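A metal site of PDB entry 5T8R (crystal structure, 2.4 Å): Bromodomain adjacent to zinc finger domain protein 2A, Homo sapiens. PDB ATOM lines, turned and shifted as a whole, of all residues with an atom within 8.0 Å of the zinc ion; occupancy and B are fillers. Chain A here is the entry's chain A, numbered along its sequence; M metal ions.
Four residues have an atom within 4 Å of the zinc ion: Cys 24, Cys 27, Cys 50 and Cys 53. The nearest printed residue that does not touch the zinc ion is Gly 26 (4.2 Å).
The side-chain sulfur (SG) of Cys 24 binds the zinc ion (2.3 Å). SG of Cys 27 binds the zinc ion (2.3 Å). The side-chain sulfur (SG) of Cys 53 binds the zinc ion, 2.3 Å away. SG of Cys 50 is bound to the zinc ion (2.3 Å).
The backbone NH (N) of Gly 26 lies close to the side-chain sulfur (SG) of Cys 24 (3.3 Å). SG of Cys 50 sits close to N of Val 52 (3.5 Å). NH1 of Arg 29 sits close to SG of Cys 27. O of Arg 29 lies within hydrogen-bond range of N of Cys 24 (3.0 Å).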
ATOM      1  N   LEU A  10      -1.313 -22.989  -0.685  1.00  0.00           N
ATOM      2  CA  LEU A  10      -1.652 -24.405  -0.928  1.00  0.00           C
ATOM      3  C   LEU A  10      -2.797 -24.949  -0.078  1.00  0.00           C
ATOM      4  O   LEU A  10      -3.503 -25.854  -0.523  1.00  0.00           O
ATOM      5  CB  LEU A  10      -0.422 -25.300  -0.722  1.00  0.00           C
ATOM      6  CG  LEU A  10       0.625 -25.291  -1.826  1.00  0.00           C
ATOM      7  CD1 LEU A  10       1.847 -26.091  -1.365  1.00  0.00           C
ATOM      8  CD2 LEU A  10       0.080 -25.866  -3.123  1.00  0.00           C
ATOM      9  N   LEU A  23       6.602 -17.860   0.423  1.00  0.00           N
ATOM     10  CA  LEU A  23       6.916 -18.412  -0.897  1.00  0.00           C
ATOM     11  C   LEU A  23       7.902 -19.574  -0.750  1.00  0.00           C
ATOM     12  O   LEU A  23       8.804 -19.535   0.097  1.00  0.00           O
ATOM     13  CB  LEU A  23       7.522 -17.351  -1.786  1.00  0.00           C
ATOM     14  CG  LEU A  23       6.708 -16.076  -2.062  1.00  0.00           C
ATOM     15  CD1 LEU A  23       7.474 -15.181  -3.027  1.00  0.00           C
ATOM     16  CD2 LEU A  23       5.318 -16.388  -2.622  1.00  0.00           C
ATOM     17  N   CYS A  24       7.716 -20.603  -1.569  1.00  0.00           N
ATOM     18  CA  CYS A  24       8.602 -21.751  -1.580  1.00  0.00           C
ATOM     19  C   CYS A  24       9.874 -21.315  -2.244  1.00  0.00           C
ATOM     20  O   CYS A  24       9.814 -20.689  -3.293  1.00  0.00           O
ATOM     21  CB  CYS A  24       8.004 -22.904  -2.342  1.00  0.00           C
ATOM     22  SG  CYS A  24       9.101 -24.349  -2.441  1.00  0.00           S
ATOM     23  N   ASP A  25      11.009 -21.644  -1.645  1.00  0.00           N
ATOM     24  CA  ASP A  25      12.311 -21.346  -2.251  1.00  0.00           C
ATOM     25  C   ASP A  25      12.629 -22.194  -3.507  1.00  0.00           C
ATOM     26  O   ASP A  25      13.485 -21.815  -4.291  1.00  0.00           O
ATOM     27  CB  ASP A  25      13.437 -21.406  -1.205  1.00  0.00           C
ATOM     28  CG  ASP A  25      13.474 -20.159  -0.327  1.00  0.00           C
ATOM     29  OD1 ASP A  25      13.721 -19.055  -0.854  1.00  0.00           O
ATOM     30  OD2 ASP A  25      13.255 -20.264   0.899  1.00  0.00           O
ATOM     31  N   GLY A  26      11.910 -23.307  -3.704  1.00  0.00           N
ATOM     32  CA  GLY A  26      12.136 -24.204  -4.827  1.00  0.00           C
ATOM     33  C   GLY A  26      11.111 -24.157  -5.960  1.00  0.00           C
ATOM     34  O   GLY A  26      11.377 -24.723  -7.018  1.00  0.00           O
ATOM     35  N   CYS A  27       9.960 -23.516  -5.761  1.00  0.00           N
ATOM     36  CA  CYS A  27       8.963 -23.392  -6.846  1.00  0.00           C
ATOM     37  C   CYS A  27       8.125 -22.118  -6.667  1.00  0.00           C
ATOM     38  O   CYS A  27       8.422 -21.283  -5.818  1.00  0.00           O
ATOM     39  CB  CYS A  27       8.096 -24.649  -6.881  1.00  0.00           C
ATOM     40  SG  CYS A  27       6.917 -24.789  -5.517  1.00  0.00           S
ATOM     41  N   ASP A  28       7.066 -21.984  -7.461  1.00  0.00           N
ATOM     42  CA  ASP A  28       6.181 -20.815  -7.403  1.00  0.00           C
ATOM     43  C   ASP A  28       4.936 -21.010  -6.497  1.00  0.00           C
ATOM     44  O   ASP A  28       3.913 -20.326  -6.673  1.00  0.00           O
ATOM     45  CB  ASP A  28       5.797 -20.404  -8.843  1.00  0.00           C
ATOM     46  CG  ASP A  28       7.031 -20.145  -9.730  1.00  0.00           C
ATOM     47  OD1 ASP A  28       8.071 -19.692  -9.175  1.00  0.00           O
ATOM     48  OD2 ASP A  28       6.985 -20.384 -10.968  1.00  0.00           O
ATOM     49  N   ARG A  29       5.036 -21.878  -5.494  1.00  0.00           N
ATOM     50  CA  ARG A  29       3.907 -22.187  -4.623  1.00  0.00           C
ATOM     51  C   ARG A  29       4.040 -21.424  -3.317  1.00  0.00           C
ATOM     52  O   ARG A  29       5.120 -20.937  -2.973  1.00  0.00           O
ATOM     53  CB  ARG A  29       3.844 -23.679  -4.303  1.00  0.00           C
ATOM     54  CG  ARG A  29       3.375 -24.535  -5.463  1.00  0.00           C
ATOM     55  CD  ARG A  29       3.452 -25.993  -5.082  1.00  0.00           C
ATOM     56  NE  ARG A  29       3.005 -26.814  -6.193  1.00  0.00           N
ATOM     57  CZ  ARG A  29       3.747 -27.111  -7.255  1.00  0.00           C
ATOM     58  NH1 ARG A  29       5.004 -26.672  -7.362  1.00  0.00           N
ATOM     59  NH2 ARG A  29       3.254 -27.877  -8.218  1.00  0.00           N
ATOM     60  N   GLY A  30       2.939 -21.322  -2.578  1.00  0.00           N
ATOM     61  CA  GLY A  30       2.904 -20.513  -1.367  1.00  0.00           C
ATOM     62  C   GLY A  30       2.137 -21.115  -0.241  1.00  0.00           C
ATOM     63  O   GLY A  30       1.367 -22.030  -0.442  1.00  0.00           O
ATOM     64  N   TRP A  48      12.981 -22.121   2.818  1.00  0.00           N
ATOM     65  CA  TRP A  48      11.794 -22.907   3.090  1.00  0.00           C
ATOM     66  C   TRP A  48      11.277 -23.539   1.801  1.00  0.00           C
ATOM     67  O   TRP A  48      11.103 -22.868   0.804  1.00  0.00           O
ATOM     68  CB  TRP A  48      10.689 -22.063   3.727  1.00  0.00           C
ATOM     69  CG  TRP A  48       9.458 -22.869   3.985  1.00  0.00           C
ATOM     70  CD1 TRP A  48       9.258 -23.771   4.991  1.00  0.00           C
ATOM     71  CD2 TRP A  48       8.274 -22.879   3.185  1.00  0.00           C
ATOM     72  NE1 TRP A  48       8.010 -24.317   4.878  1.00  0.00           N
ATOM     73  CE2 TRP A  48       7.380 -23.800   3.776  1.00  0.00           C
ATOM     74  CE3 TRP A  48       7.868 -22.191   2.044  1.00  0.00           C
ATOM     75  CZ2 TRP A  48       6.101 -24.067   3.248  1.00  0.00           C
ATOM     76  CZ3 TRP A  48       6.593 -22.440   1.500  1.00  0.00           C
ATOM     77  CH2 TRP A  48       5.726 -23.374   2.108  1.00  0.00           C
ATOM     78  N   PHE A  49      11.000 -24.847   1.876  1.00  0.00           N
ATOM     79  CA  PHE A  49      10.522 -25.626   0.742  1.00  0.00           C
ATOM     80  C   PHE A  49       9.137 -26.192   0.979  1.00  0.00           C
ATOM     81  O   PHE A  49       8.858 -26.766   2.031  1.00  0.00           O
ATOM     82  CB  PHE A  49      11.525 -26.727   0.432  1.00  0.00           C
ATOM     83  CG  PHE A  49      12.871 -26.188   0.051  1.00  0.00           C
ATOM     84  CD1 PHE A  49      13.111 -25.722  -1.240  1.00  0.00           C
ATOM     85  CD2 PHE A  49      13.891 -26.089   1.000  1.00  0.00           C
ATOM     86  CE1 PHE A  49      14.339 -25.196  -1.596  1.00  0.00           C
ATOM     87  CE2 PHE A  49      15.130 -25.571   0.643  1.00  0.00           C
ATOM     88  CZ  PHE A  49      15.350 -25.119  -0.650  1.00  0.00           C
ATOM     89  N   CYS A  50       8.262 -26.049  -0.005  1.00  0.00           N
ATOM     90  CA  CYS A  50       6.924 -26.623   0.104  1.00  0.00           C
ATOM     91  C   CYS A  50       6.949 -28.177   0.023  1.00  0.00           C
ATOM     92  O   CYS A  50       7.969 -28.801  -0.296  1.00  0.00           O
ATOM     93  CB  CYS A  50       6.008 -26.027  -0.952  1.00  0.00           C
ATOM     94  SG  CYS A  50       6.136 -26.823  -2.554  1.00  0.00           S
ATOM     95  N   THR A  51       5.797 -28.782   0.293  1.00  0.00           N
ATOM     96  CA  THR A  51       5.724 -30.244   0.374  1.00  0.00           C
ATOM     97  C   THR A  51       5.912 -30.940  -0.993  1.00  0.00           C
ATOM     98  O   THR A  51       6.439 -32.067  -1.083  1.00  0.00           O
ATOM     99  CB  THR A  51       4.432 -30.661   1.049  1.00  0.00           C
ATOM    100  OG1 THR A  51       3.319 -30.091   0.351  1.00  0.00           O
ATOM    101  CG2 THR A  51       4.426 -30.177   2.506  1.00  0.00           C
ATOM    102  N   VAL A  52       5.537 -30.241  -2.060  1.00  0.00           N
ATOM    103  CA  VAL A  52       5.775 -30.729  -3.408  1.00  0.00           C
ATOM    104  C   VAL A  52       7.274 -30.788  -3.699  1.00  0.00           C
ATOM    105  O   VAL A  52       7.740 -31.741  -4.339  1.00  0.00           O
ATOM    106  CB  VAL A  52       5.063 -29.852  -4.462  1.00  0.00           C
ATOM    107  CG1 VAL A  52       5.284 -30.425  -5.858  1.00  0.00           C
ATOM    108  CG2 VAL A  52       3.565 -29.725  -4.146  1.00  0.00           C
ATOM    109  N   CYS A  53       8.021 -29.787  -3.225  1.00  0.00           N
ATOM    110  CA  CYS A  53       9.487 -29.779  -3.322  1.00  0.00           C
ATOM    111  C   CYS A  53      10.187 -30.806  -2.429  1.00  0.00           C
ATOM    112  O   CYS A  53      11.209 -31.386  -2.834  1.00  0.00           O
ATOM    113  CB  CYS A  53      10.056 -28.384  -3.050  1.00  0.00           C
ATOM    114  SG  CYS A  53       9.666 -27.217  -4.382  1.00  0.00           S
ATOM    115  N   LEU A  54       9.647 -31.038  -1.234  1.00  0.00           N
ATOM    116  CA  LEU A  54      10.118 -32.153  -0.396  1.00  0.00           C
ATOM    117  C   LEU A  54      10.010 -33.515  -1.088  1.00  0.00           C
ATOM    118  O   LEU A  54      10.891 -34.367  -0.916  1.00  0.00           O
ATOM    119  CB  LEU A  54       9.351 -32.237   0.929  1.00  0.00           C
ATOM    120  CG  LEU A  54       9.575 -31.145   1.967  1.00  0.00           C
ATOM    121  CD1 LEU A  54       9.098 -31.664   3.325  1.00  0.00           C
ATOM    122  CD2 LEU A  54      11.021 -30.667   2.055  1.00  0.00           C
ATOM    123  N   GLN A  56      10.437 -34.107  -4.186  1.00  0.00           N
ATOM    124  CA  GLN A  56      11.515 -34.249  -5.196  1.00  0.00           C
ATOM    125  C   GLN A  56      12.915 -34.427  -4.610  1.00  0.00           C
ATOM    126  O   GLN A  56      13.850 -34.712  -5.364  1.00  0.00           O
ATOM    127  CB  GLN A  56      11.566 -33.037  -6.146  1.00  0.00           C
ATOM    128  CG  GLN A  56      10.231 -32.553  -6.699  1.00  0.00           C
ATOM    129  CD  GLN A  56       9.369 -33.667  -7.283  1.00  0.00           C
ATOM    130  OE1 GLN A  56       9.887 -34.586  -7.946  1.00  0.00           O
ATOM    131  NE2 GLN A  56       8.060 -33.590  -7.048  1.00  0.00           N
HETATM  132 ZN    ZN M   1       7.911 -25.838  -3.727  1.00  0.00          ZN
